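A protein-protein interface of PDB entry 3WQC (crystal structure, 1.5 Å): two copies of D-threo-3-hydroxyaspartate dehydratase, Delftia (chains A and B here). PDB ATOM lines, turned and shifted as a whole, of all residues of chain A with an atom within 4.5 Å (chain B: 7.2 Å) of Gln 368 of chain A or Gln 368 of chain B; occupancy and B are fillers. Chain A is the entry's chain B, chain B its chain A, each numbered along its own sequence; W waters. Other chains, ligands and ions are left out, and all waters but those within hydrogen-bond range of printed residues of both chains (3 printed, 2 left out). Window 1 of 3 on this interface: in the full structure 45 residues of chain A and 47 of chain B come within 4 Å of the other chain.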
ATOM      1  N   TRP A 290      -1.236  15.025  37.290  1.00  0.00           N
ATOM      2  CA  TRP A 290      -1.609  16.292  36.630  1.00  0.00           C
ATOM      3  C   TRP A 290      -1.900  16.090  35.169  1.00  0.00           C
ATOM      4  O   TRP A 290      -2.629  16.931  34.555  1.00  0.00           O
ATOM      5  CB  TRP A 290      -0.599  17.417  36.835  1.00  0.00           C
ATOM      6  CG  TRP A 290       0.797  17.134  36.332  1.00  0.00           C
ATOM      7  CD1 TRP A 290       1.922  16.872  37.095  1.00  0.00           C
ATOM      8  CD2 TRP A 290       1.232  17.101  34.896  1.00  0.00           C
ATOM      9  NE1 TRP A 290       3.003  16.649  36.254  1.00  0.00           N
ATOM     10  CE2 TRP A 290       2.617  16.750  34.893  1.00  0.00           C
ATOM     11  CE3 TRP A 290       0.579  17.317  33.642  1.00  0.00           C
ATOM     12  CZ2 TRP A 290       3.350  16.622  33.726  1.00  0.00           C
ATOM     13  CZ3 TRP A 290       1.308  17.151  32.459  1.00  0.00           C
ATOM     14  CH2 TRP A 290       2.684  16.797  32.490  1.00  0.00           C
ATOM     15  N   MET A 291      -1.486  14.944  34.567  1.00  0.00           N
ATOM     16  CA  MET A 291      -1.924  14.761  33.163  1.00  0.00           C
ATOM     17  C   MET A 291      -3.450  14.546  33.121  1.00  0.00           C
ATOM     18  O   MET A 291      -4.074  14.935  32.144  1.00  0.00           O
ATOM     19  CB  MET A 291      -1.209  13.567  32.522  1.00  0.00           C
ATOM     20  CG  MET A 291      -1.439  13.434  30.983  1.00  0.00           C
ATOM     21  SD  MET A 291      -0.816  14.881  30.057  1.00  0.00           S
ATOM     22  CE  MET A 291       0.953  14.508  30.112  1.00  0.00           C
ATOM     23  N   ALA A 292      -4.068  13.958  34.153  1.00  0.00           N
ATOM     24  CA  ALA A 292      -5.532  13.844  34.210  1.00  0.00           C
ATOM     25  C   ALA A 292      -6.144  15.125  34.746  1.00  0.00           C
ATOM     26  O   ALA A 292      -7.165  15.619  34.205  1.00  0.00           O
ATOM     27  CB  ALA A 292      -5.919  12.679  35.109  1.00  0.00           C
ATOM     28  N   SER A 294      -4.874  18.174  35.050  1.00  0.00           N
ATOM     29  CA  SER A 294      -4.215  19.393  34.643  1.00  0.00           C
ATOM     30  C   SER A 294      -3.389  19.979  35.809  1.00  0.00           C
ATOM     31  O   SER A 294      -3.631  19.633  37.006  1.00  0.00           O
ATOM     32  CB  SER A 294      -5.087  20.521  34.041  1.00  0.00           C
ATOM     33  OG  SER A 294      -5.622  21.357  35.083  1.00  0.00           O
ATOM     34  N   ALA A 364      -9.815  23.450  32.327  1.00  0.00           N
ATOM     35  CA  ALA A 364      -8.412  22.943  32.242  1.00  0.00           C
ATOM     36  C   ALA A 364      -8.396  21.424  32.337  1.00  0.00           C
ATOM     37  O   ALA A 364      -7.745  20.705  31.556  1.00  0.00           O
ATOM     38  CB  ALA A 364      -7.597  23.558  33.359  1.00  0.00           C
ATOM     39  N   THR A 365      -9.202  20.844  33.289  1.00  0.00           N
ATOM     40  CA  THR A 365      -9.224  19.346  33.413  1.00  0.00           C
ATOM     41  C   THR A 365      -9.843  18.754  32.177  1.00  0.00           C
ATOM     42  O   THR A 365      -9.274  17.755  31.647  1.00  0.00           O
ATOM     43  CB  THR A 365     -10.042  18.946  34.663  1.00  0.00           C
ATOM     44  OG1 THR A 365      -9.382  19.492  35.830  1.00  0.00           O
ATOM     45  CG2 THR A 365     -10.251  17.427  34.736  1.00  0.00           C
ATOM     46  N   GLY A 366     -10.923  19.325  31.627  1.00  0.00           N
ATOM     47  CA  GLY A 366     -11.580  18.671  30.486  1.00  0.00           C
ATOM     48  C   GLY A 366     -10.616  18.558  29.290  1.00  0.00           C
ATOM     49  O   GLY A 366     -10.647  17.570  28.527  1.00  0.00           O
ATOM     50  N   ALA A 367      -9.742  19.562  29.112  1.00  0.00           N
ATOM     51  CA  ALA A 367      -8.886  19.609  27.932  1.00  0.00           C
ATOM     52  C   ALA A 367      -7.833  18.465  27.939  1.00  0.00           C
ATOM     53  O   ALA A 367      -7.179  18.184  26.929  1.00  0.00           O
ATOM     54  CB  ALA A 367      -8.154  20.957  27.875  1.00  0.00           C
ATOM     55  N   GLN A 368      -7.628  17.847  29.108  1.00  0.00           N
ATOM     56  CA  GLN A 368      -6.683  16.718  29.198  1.00  0.00           C
ATOM     57  C   GLN A 368      -7.234  15.420  28.614  1.00  0.00           C
ATOM     58  O   GLN A 368      -6.470  14.445  28.449  1.00  0.00           O
ATOM     59  CB  GLN A 368      -6.307  16.505  30.661  1.00  0.00           C
ATOM     60  CG  GLN A 368      -5.632  17.736  31.291  1.00  0.00           C
ATOM     61  CD  GLN A 368      -4.363  18.162  30.527  1.00  0.00           C
ATOM     62  OE1 GLN A 368      -4.400  19.080  29.635  1.00  0.00           O
ATOM     63  NE2 GLN A 368      -3.233  17.494  30.837  1.00  0.00           N
ATOM     64  N   PHE A 369      -8.513  15.390  28.272  1.00  0.00           N
ATOM     65  CA  PHE A 369      -9.144  14.134  27.807  1.00  0.00           C
ATOM     66  C   PHE A 369      -9.609  14.225  26.362  1.00  0.00           C
ATOM     67  O   PHE A 369     -10.245  15.208  25.983  1.00  0.00           O
ATOM     68  CB  PHE A 369     -10.355  13.794  28.675  1.00  0.00           C
ATOM     69  CG  PHE A 369      -9.950  13.470  30.078  1.00  0.00           C
ATOM     70  CD1 PHE A 369      -9.745  14.483  31.030  1.00  0.00           C
ATOM     71  CD2 PHE A 369      -9.755  12.130  30.466  1.00  0.00           C
ATOM     72  CE1 PHE A 369      -9.308  14.178  32.340  1.00  0.00           C
ATOM     73  CE2 PHE A 369      -9.308  11.809  31.759  1.00  0.00           C
ATOM     74  CZ  PHE A 369      -9.097  12.832  32.716  1.00  0.00           C
ATOM     75  N   PRO A 370      -9.426  13.132  25.592  1.00  0.00           N
ATOM     76  CA  PRO A 370      -9.989  13.079  24.244  1.00  0.00           C
ATOM     77  C   PRO A 370     -11.523  13.080  24.299  1.00  0.00           C
ATOM     78  O   PRO A 370     -12.135  13.457  23.294  1.00  0.00           O
ATOM     79  CB  PRO A 370      -9.497  11.735  23.685  1.00  0.00           C
ATOM     80  CG  PRO A 370      -8.210  11.457  24.462  1.00  0.00           C
ATOM     81  CD  PRO A 370      -8.431  12.025  25.848  1.00  0.00           C
ATOM     82  N   HIS A 388      -9.368  18.711  20.771  1.00  0.00           N
ATOM     83  CA  HIS A 388      -8.023  19.013  21.293  1.00  0.00           C
ATOM     84  C   HIS A 388      -7.249  19.764  20.227  1.00  0.00           C
ATOM     85  O   HIS A 388      -7.262  19.402  19.059  1.00  0.00           O
ATOM     86  CB  HIS A 388      -7.331  17.628  21.573  1.00  0.00           C
ATOM     87  CG  HIS A 388      -6.009  17.753  22.215  1.00  0.00           C
ATOM     88  ND1 HIS A 388      -4.907  17.070  21.737  1.00  0.00           N
ATOM     89  CD2 HIS A 388      -5.623  18.423  23.368  1.00  0.00           C
ATOM     90  CE1 HIS A 388      -3.851  17.293  22.629  1.00  0.00           C
ATOM     91  NE2 HIS A 388      -4.307  18.124  23.633  1.00  0.00           N
ATOM     92  N   TRP A 390      -5.676  23.009  17.829  1.00  0.00           N
ATOM     93  CA  TRP A 390      -6.044  24.209  17.086  1.00  0.00           C
ATOM     94  C   TRP A 390      -6.242  23.879  15.634  1.00  0.00           C
ATOM     95  O   TRP A 390      -5.963  22.736  15.223  1.00  0.00           O
ATOM     96  CB  TRP A 390      -4.949  25.292  17.237  1.00  0.00           C
ATOM     97  CG  TRP A 390      -4.832  25.786  18.649  1.00  0.00           C
ATOM     98  CD1 TRP A 390      -5.460  26.886  19.174  1.00  0.00           C
ATOM     99  CD2 TRP A 390      -4.092  25.146  19.766  1.00  0.00           C
ATOM    100  NE1 TRP A 390      -5.174  26.997  20.534  1.00  0.00           N
ATOM    101  CE2 TRP A 390      -4.332  25.946  20.929  1.00  0.00           C
ATOM    102  CE3 TRP A 390      -3.267  23.998  19.855  1.00  0.00           C
ATOM    103  CZ2 TRP A 390      -3.839  25.594  22.209  1.00  0.00           C
ATOM    104  CZ3 TRP A 390      -2.778  23.669  21.155  1.00  0.00           C
ATOM    105  CH2 TRP A 390      -3.059  24.455  22.299  1.00  0.00           C
ATOM    106  OXT TRP A 390      -6.626  24.811  14.886  1.00  0.00           O
ATOM    107  N   ALA B  23       3.652  23.867  18.620  1.00  0.00           N
ATOM    108  CA  ALA B  23       4.757  23.333  19.393  1.00  0.00           C
ATOM    109  C   ALA B  23       5.875  23.019  18.447  1.00  0.00           C
ATOM    110  O   ALA B  23       5.740  22.059  17.677  1.00  0.00           O
ATOM    111  CB  ALA B  23       4.302  22.129  20.216  1.00  0.00           C
ATOM    112  N   GLY B 289      -2.036  30.998  25.334  1.00  0.00           N
ATOM    113  CA  GLY B 289      -2.406  31.058  26.735  1.00  0.00           C
ATOM    114  C   GLY B 289      -2.038  29.758  27.462  1.00  0.00           C
ATOM    115  O   GLY B 289      -1.155  29.012  26.979  1.00  0.00           O
ATOM    116  N   TRP B 290      -2.691  29.468  28.583  1.00  0.00           N
ATOM    117  CA  TRP B 290      -2.340  28.228  29.302  1.00  0.00           C
ATOM    118  C   TRP B 290      -2.830  27.031  28.484  1.00  0.00           C
ATOM    119  O   TRP B 290      -2.310  25.906  28.748  1.00  0.00           O
ATOM    120  CB  TRP B 290      -2.790  28.186  30.786  1.00  0.00           C
ATOM    121  CG  TRP B 290      -4.273  28.274  30.979  1.00  0.00           C
ATOM    122  CD1 TRP B 290      -4.973  29.356  31.515  1.00  0.00           C
ATOM    123  CD2 TRP B 290      -5.281  27.204  30.754  1.00  0.00           C
ATOM    124  NE1 TRP B 290      -6.298  29.052  31.605  1.00  0.00           N
ATOM    125  CE2 TRP B 290      -6.564  27.784  31.102  1.00  0.00           C
ATOM    126  CE3 TRP B 290      -5.239  25.868  30.266  1.00  0.00           C
ATOM    127  CZ2 TRP B 290      -7.752  27.093  30.970  1.00  0.00           C
ATOM    128  CZ3 TRP B 290      -6.463  25.192  30.107  1.00  0.00           C
ATOM    129  CH2 TRP B 290      -7.704  25.787  30.470  1.00  0.00           C
ATOM    130  N   MET B 291      -3.811  27.116  27.566  1.00  0.00           N
ATOM    131  CA  MET B 291      -4.169  25.913  26.760  1.00  0.00           C
ATOM    132  C   MET B 291      -2.920  25.515  25.946  1.00  0.00           C
ATOM    133  O   MET B 291      -2.761  24.352  25.645  1.00  0.00           O
ATOM    134  CB  MET B 291      -5.399  26.168  25.904  1.00  0.00           C
ATOM    135  CG  MET B 291      -5.883  24.907  25.242  1.00  0.00           C
ATOM    136  SD  MET B 291      -6.442  23.609  26.446  1.00  0.00           S
ATOM    137  CE  MET B 291      -8.021  24.329  26.967  1.00  0.00           C
ATOM    138  N   ALA B 292      -2.109  26.481  25.480  1.00  0.00           N
ATOM    139  CA  ALA B 292      -0.882  26.176  24.721  1.00  0.00           C
ATOM    140  C   ALA B 292       0.246  25.826  25.700  1.00  0.00           C
ATOM    141  O   ALA B 292       0.989  24.821  25.495  1.00  0.00           O
ATOM    142  CB  ALA B 292      -0.464  27.377  23.866  1.00  0.00           C
ATOM    143  N   MET B 293       0.481  26.640  26.725  1.00  0.00           N
ATOM    144  CA  MET B 293       1.700  26.418  27.514  1.00  0.00           C
ATOM    145  C   MET B 293       1.481  25.322  28.588  1.00  0.00           C
ATOM    146  O   MET B 293       2.498  24.832  29.148  1.00  0.00           O
ATOM    147  CB  MET B 293       2.063  27.706  28.301  1.00  0.00           C
ATOM    148  CG  MET B 293       2.385  28.904  27.399  1.00  0.00           C
ATOM    149  SD  MET B 293       3.488  28.537  25.990  1.00  0.00           S
ATOM    150  CE  MET B 293       4.981  27.909  26.842  1.00  0.00           C
ATOM    151  N   SER B 294       0.218  25.001  28.918  1.00  0.00           N
ATOM    152  CA  SER B 294      -0.225  24.271  30.100  1.00  0.00           C
ATOM    153  C   SER B 294      -0.214  25.220  31.297  1.00  0.00           C
ATOM    154  O   SER B 294       0.452  26.287  31.287  1.00  0.00           O
ATOM    155  CB  SER B 294       0.630  22.964  30.456  1.00  0.00           C
ATOM    156  OG  SER B 294       1.753  23.312  31.237  1.00  0.00           O
ATOM    157  N   ARG B 295      -0.879  24.798  32.373  1.00  0.00           N
ATOM    158  CA  ARG B 295      -0.869  25.565  33.679  1.00  0.00           C
ATOM    159  C   ARG B 295       0.413  25.281  34.458  1.00  0.00           C
ATOM    160  O   ARG B 295       0.522  25.799  35.577  1.00  0.00           O
ATOM    161  CB  ARG B 295      -2.076  25.125  34.502  1.00  0.00           C
ATOM    162  CG  ARG B 295      -3.337  25.885  34.065  1.00  0.00           C
ATOM    163  CD  ARG B 295      -3.192  27.409  34.455  1.00  0.00           C
ATOM    164  NE  ARG B 295      -4.506  27.927  34.801  1.00  0.00           N
ATOM    165  CZ  ARG B 295      -4.794  29.220  34.940  1.00  0.00           C
ATOM    166  NH1 ARG B 295      -3.891  30.135  34.649  1.00  0.00           N
ATOM    167  NH2 ARG B 295      -6.051  29.548  35.311  1.00  0.00           N
ATOM    168  N   ALA B 362       8.613  20.775  29.816  1.00  0.00           N
ATOM    169  CA  ALA B 362       8.413  20.314  28.432  1.00  0.00           C
ATOM    170  C   ALA B 362       7.301  19.231  28.370  1.00  0.00           C
ATOM    171  O   ALA B 362       6.477  19.245  27.446  1.00  0.00           O
ATOM    172  CB  ALA B 362       9.695  19.778  27.826  1.00  0.00           C
ATOM    173  N   CYS B 363       7.223  18.351  29.369  1.00  0.00           N
ATOM    174  CA  CYS B 363       6.281  17.224  29.301  1.00  0.00           C
ATOM    175  C   CYS B 363       4.843  17.766  29.385  1.00  0.00           C
ATOM    176  O   CYS B 363       3.910  17.226  28.754  1.00  0.00           O
ATOM    177  CB  CYS B 363       6.497  16.348  30.562  1.00  0.00           C
ATOM    178  SG  CYS B 363       8.289  15.985  30.869  1.00  0.00           S
ATOM    179  N   ALA B 364       4.668  18.862  30.180  1.00  0.00           N
ATOM    180  CA  ALA B 364       3.317  19.426  30.351  1.00  0.00           C
ATOM    181  C   ALA B 364       2.897  20.219  29.083  1.00  0.00           C
ATOM    182  O   ALA B 364       1.766  20.085  28.610  1.00  0.00           O
ATOM    183  CB  ALA B 364       3.249  20.308  31.603  1.00  0.00           C
ATOM    184  N   THR B 365       3.847  21.076  28.575  1.00  0.00           N
ATOM    185  CA  THR B 365       3.482  21.882  27.391  1.00  0.00           C
ATOM    186  C   THR B 365       3.176  20.957  26.203  1.00  0.00           C
ATOM    187  O   THR B 365       2.227  21.139  25.471  1.00  0.00           O
ATOM    188  CB  THR B 365       4.617  22.808  27.061  1.00  0.00           C
ATOM    189  OG1 THR B 365       4.719  23.739  28.162  1.00  0.00           O
ATOM    190  CG2 THR B 365       4.395  23.569  25.767  1.00  0.00           C
ATOM    191  N   GLY B 366       4.031  19.932  26.016  1.00  0.00           N
ATOM    192  CA  GLY B 366       3.898  19.059  24.791  1.00  0.00           C
ATOM    193  C   GLY B 366       2.532  18.408  24.804  1.00  0.00           C
ATOM    194  O   GLY B 366       1.931  18.235  23.726  1.00  0.00           O
ATOM    195  N   ALA B 367       2.031  18.002  25.997  1.00  0.00           N
ATOM    196  CA  ALA B 367       0.757  17.321  26.048  1.00  0.00           C
ATOM    197  C   ALA B 367      -0.449  18.156  25.628  1.00  0.00           C
ATOM    198  O   ALA B 367      -1.543  17.606  25.329  1.00  0.00           O
ATOM    199  CB  ALA B 367       0.503  16.754  27.435  1.00  0.00           C
ATOM    200  N   GLN B 368      -0.257  19.490  25.540  1.00  0.00           N
ATOM    201  CA  GLN B 368      -1.335  20.338  25.065  1.00  0.00           C
ATOM    202  C   GLN B 368      -1.532  20.271  23.548  1.00  0.00           C
ATOM    203  O   GLN B 368      -2.520  20.833  23.036  1.00  0.00           O
ATOM    204  CB  GLN B 368      -1.012  21.781  25.502  1.00  0.00           C
ATOM    205  CG  GLN B 368      -0.977  21.929  27.048  1.00  0.00           C
ATOM    206  CD  GLN B 368      -2.246  21.433  27.742  1.00  0.00           C
ATOM    207  OE1 GLN B 368      -2.355  20.250  28.126  1.00  0.00           O
ATOM    208  NE2 GLN B 368      -3.180  22.341  27.995  1.00  0.00           N
ATOM    209  N   PHE B 369      -0.610  19.642  22.792  1.00  0.00           N
ATOM    210  CA  PHE B 369      -0.653  19.713  21.310  1.00  0.00           C
ATOM    211  C   PHE B 369      -0.898  18.331  20.728  1.00  0.00           C
ATOM    212  O   PHE B 369      -0.277  17.348  21.177  1.00  0.00           O
ATOM    213  CB  PHE B 369       0.709  20.233  20.765  1.00  0.00           C
ATOM    214  CG  PHE B 369       0.891  21.680  21.128  1.00  0.00           C
ATOM    215  CD1 PHE B 369       1.425  22.048  22.346  1.00  0.00           C
ATOM    216  CD2 PHE B 369       0.464  22.665  20.211  1.00  0.00           C
ATOM    217  CE1 PHE B 369       1.544  23.415  22.687  1.00  0.00           C
ATOM    218  CE2 PHE B 369       0.600  24.026  20.550  1.00  0.00           C
ATOM    219  CZ  PHE B 369       1.142  24.392  21.761  1.00  0.00           C
ATOM    220  N   PRO B 370      -1.707  18.263  19.689  1.00  0.00           N
ATOM    221  CA  PRO B 370      -1.826  17.015  18.932  1.00  0.00           C
ATOM    222  C   PRO B 370      -0.551  16.563  18.254  1.00  0.00           C
ATOM    223  O   PRO B 370      -0.425  15.357  17.959  1.00  0.00           O
ATOM    224  CB  PRO B 370      -2.928  17.347  17.865  1.00  0.00           C
ATOM    225  CG  PRO B 370      -3.706  18.494  18.511  1.00  0.00           C
ATOM    226  CD  PRO B 370      -2.679  19.305  19.271  1.00  0.00           C
ATOM    227  N   ALA B 371       0.346  17.491  17.988  1.00  0.00           N
ATOM    228  CA  ALA B 371       1.520  17.187  17.189  1.00  0.00           C
ATOM    229  C   ALA B 371       2.570  18.253  17.440  1.00  0.00           C
ATOM    230  O   ALA B 371       2.222  19.418  17.852  1.00  0.00           O
ATOM    231  CB  ALA B 371       1.227  17.127  15.680  1.00  0.00           C
ATOM    232  N   ARG B 386       1.810  13.279  18.170  1.00  0.00           N
ATOM    233  CA  ARG B 386       2.032  12.666  19.484  1.00  0.00           C
ATOM    234  C   ARG B 386       0.730  12.186  20.063  1.00  0.00           C
ATOM    235  O   ARG B 386      -0.378  12.599  19.647  1.00  0.00           O
ATOM    236  CB  ARG B 386       2.808  13.614  20.401  1.00  0.00           C
ATOM    237  CG  ARG B 386       2.036  14.899  20.672  1.00  0.00           C
ATOM    238  CD  ARG B 386       2.516  15.504  21.998  1.00  0.00           C
ATOM    239  NE  ARG B 386       2.042  14.714  23.136  1.00  0.00           N
ATOM    240  CZ  ARG B 386       2.615  14.691  24.335  1.00  0.00           C
ATOM    241  NH1 ARG B 386       1.995  14.070  25.356  1.00  0.00           N
ATOM    242  NH2 ARG B 386       3.831  15.248  24.583  1.00  0.00           N
ATOM    243  N   HIS B 388      -2.333  11.600  22.930  1.00  0.00           N
ATOM    244  CA  HIS B 388      -3.150  12.256  23.954  1.00  0.00           C
ATOM    245  C   HIS B 388      -4.046  11.204  24.558  1.00  0.00           C
ATOM    246  O   HIS B 388      -4.659  10.407  23.854  1.00  0.00           O
ATOM    247  CB  HIS B 388      -4.027  13.314  23.171  1.00  0.00           C
ATOM    248  CG  HIS B 388      -4.845  14.160  24.067  1.00  0.00           C
ATOM    249  ND1 HIS B 388      -6.171  14.429  23.771  1.00  0.00           N
ATOM    250  CD2 HIS B 388      -4.495  14.929  25.147  1.00  0.00           C
ATOM    251  CE1 HIS B 388      -6.648  15.336  24.702  1.00  0.00           C
ATOM    252  NE2 HIS B 388      -5.594  15.676  25.520  1.00  0.00           N
ATOM    253  N   GLY B 389      -4.205  11.265  25.862  1.00  0.00           N
ATOM    254  CA  GLY B 389      -5.163  10.444  26.559  1.00  0.00           C
ATOM    255  C   GLY B 389      -4.661   9.081  27.038  1.00  0.00           C
ATOM    256  O   GLY B 389      -3.464   8.908  27.214  1.00  0.00           O
ATOM    257  N   TRP B 390      -5.612   8.171  27.242  1.00  0.00           N
ATOM    258  CA  TRP B 390      -5.321   6.872  27.883  1.00  0.00           C
ATOM    259  C   TRP B 390      -5.961   5.776  27.121  1.00  0.00           C
ATOM    260  O   TRP B 390      -6.858   5.992  26.256  1.00  0.00           O
ATOM    261  CB  TRP B 390      -5.892   6.857  29.345  1.00  0.00           C
ATOM    262  CG  TRP B 390      -5.161   7.819  30.212  1.00  0.00           C
ATOM    263  CD1 TRP B 390      -4.082   7.562  31.052  1.00  0.00           C
ATOM    264  CD2 TRP B 390      -5.422   9.259  30.322  1.00  0.00           C
ATOM    265  NE1 TRP B 390      -3.607   8.723  31.628  1.00  0.00           N
ATOM    266  CE2 TRP B 390      -4.409   9.783  31.233  1.00  0.00           C
ATOM    267  CE3 TRP B 390      -6.394  10.143  29.784  1.00  0.00           C
ATOM    268  CZ2 TRP B 390      -4.378  11.131  31.615  1.00  0.00           C
ATOM    269  CZ3 TRP B 390      -6.308  11.517  30.119  1.00  0.00           C
ATOM    270  CH2 TRP B 390      -5.295  12.001  30.979  1.00  0.00           C
ATOM    271  OXT TRP B 390      -5.642   4.593  27.444  1.00  0.00           O
HETATM  272  O   HOH W   1      -5.378  21.565  30.248  1.00  0.00           O
HETATM  273  O   HOH W   2      -2.758  12.570  27.856  1.00  0.00           O
HETATM  274  O   HOH W   3      -0.566  19.263  29.974  1.00  0.00           O
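Hydrophobic or aromatic side chains of chain B within 4 Å of the printed part of chain A: Trp 290, Met 291, Ala 364, Ala 367, Phe 369, Pro 370, His 388 and Trp 390.
Of the 13 printed residues of chain A, 10 touch a printed residue of chain B.
Among the printed residues, no Asp or Glu carboxylate lies within 4 Å of a Lys or Arg side-chain nitrogen of the other chain.
O of Met 291 of chain B sits close to NE2 of Gln 368 of chain B, at 3.1 Å.
O of Met 291 of chain A is in hydrogen-bond range of NE2 of Gln 368 of chain A (3.0 Å).
N of Arg 386 of chain B sits at hydrogen-bond distance from O of Pro 370 of chain B (3.1 Å).
Printed residues of chain B within 4 Å of Ala 364 of chain A: Trp 290.
Printed residues of chain B within 4 Å of Gln 368 of chain A: Gln 368 (2.8 Å), His 388 (3.3 Å) and Trp 390 (3.4 Å).
Printed residues of chain B within 4 Å of Phe 369 of chain A: His 388 and Trp 390.
Ala 23 of chain B touches none of the printed residues of chain A.
Printed residues of chain A within 4 Å of Met 291 of chain B: Ala 367 (3.5 Å) and Trp 390 (3.4 Å).
Of the printed residues of chain A, Ala 364 of chain B touches Trp 290 (3.4 Å).
Printed residues of chain A within 4 Å of Gln 368 of chain B: Gln 368 (2.8 Å), His 388 (3.3 Å) and Trp 390 (3.4 Å).
Of the printed residues of chain A, Gly 389 of chain B touches Pro 370.
The nearest printed residue of chain B that does not touch Gln 368 of chain A is Gly 389 of chain B (4.6 Å).
Trp 290 of chain A touches Ala 364 of chain B, and with the chains exchanged Ala 364 of chain A touches Trp 290 of chain B.
Met 291 of chain A touches Trp 390 of chain B, and with the chains exchanged Trp 390 of chain A touches Met 291 of chain B.
Ala 292 of chain A touches Trp 390 of chain B, and with the chains exchanged Trp 390 of chain A touches Ala 292 of chain B.
Pro 370 of chain A touches His 388 of chain B, and with the chains exchanged His 388 of chain A touches Pro 370 of chain B.
Positions printed for both chains: 290, 291, 292, 294, 364, 365, 366, 367, 368, 369, 370, 388 and 390.
Of the 24 pairs that touch across the chains among the printed residues, 22 have their exchanged pair printed and touching as well.
Cys 363 of chain B touches Trp 290 of chain A (C to CH2, 3.9 Å).
Ala 364 of chain B touches Trp 290 of chain A (CA to CH2, 3.4 Å).
Met 291 of chain A touches Trp 390 of chain B.
Trp 390 of chain B touches Ala 292 of chain A (CH2 to CA, 3.7 Å).
CA of Ala 364 of chain A touches CH2 of Trp 290 of chain B, at 3.4 Å.
Trp 390 of chain B touches Gln 368 of chain A.
N of Pro 370 of chain A touches CE1 of His 388 of chain B, at 3.7 Å.
CA of Gly 389 of chain B touches CD of Pro 370 of chain A, at 3.7 Å.
C of Phe 369 of chain B touches CE1 of His 388 of chain A, 3.7 Å away.
Trp 390 of chain A touches Ala 292 of chain B.
A ring nitrogen (NE2) of His 388 of chain A is in hydrogen-bond range of the backbone carbonyl oxygen (O) of Ala 367 of chain B, 3.3 Å away.
A ring nitrogen (NE2) of His 388 of chain A lies within hydrogen-bond range of the backbone carbonyl oxygen (O) of Gln 368 of chain B.
The side-chain amide oxygen (OE1) of Gln 368 of chain B lies close to the side-chain amide oxygen (OE1) of Gln 368 of chain A.
NE2 of His 388 of chain B is in hydrogen-bond range of NE2 of His 388 of chain A (3.3 Å).
NE2 of His 388 of chain B is in hydrogen-bond range of O of Gln 368 of chain A, at 3.3 Å.
A ring nitrogen (NE2) of His 388 of chain B sits at hydrogen-bond distance from the backbone carbonyl oxygen (O) of Ala 367 of chain A (3.3 Å).
Water W1 lies within hydrogen-bond range of OE1 of Gln 368 of chain A (2.7 Å), O of Ala 364 of chain A (2.8 Å) and NE2 of Gln 368 of chain B (3.2 Å).
Water W3 lies within hydrogen-bond range of the side-chain amide oxygen (OE1) of Gln 368 of chain B (2.8 Å), the backbone carbonyl oxygen (O) of Ala 364 of chain B (2.8 Å) and the side-chain amide nitrogen (NE2) of Gln 368 of chain A (3.3 Å).
Water W2 bridges the backbone NH (N) of Gly 389 of chain B (2.8 Å) and the side-chain sulfur (SD) of Met 291 of chain A (3.7 Å).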
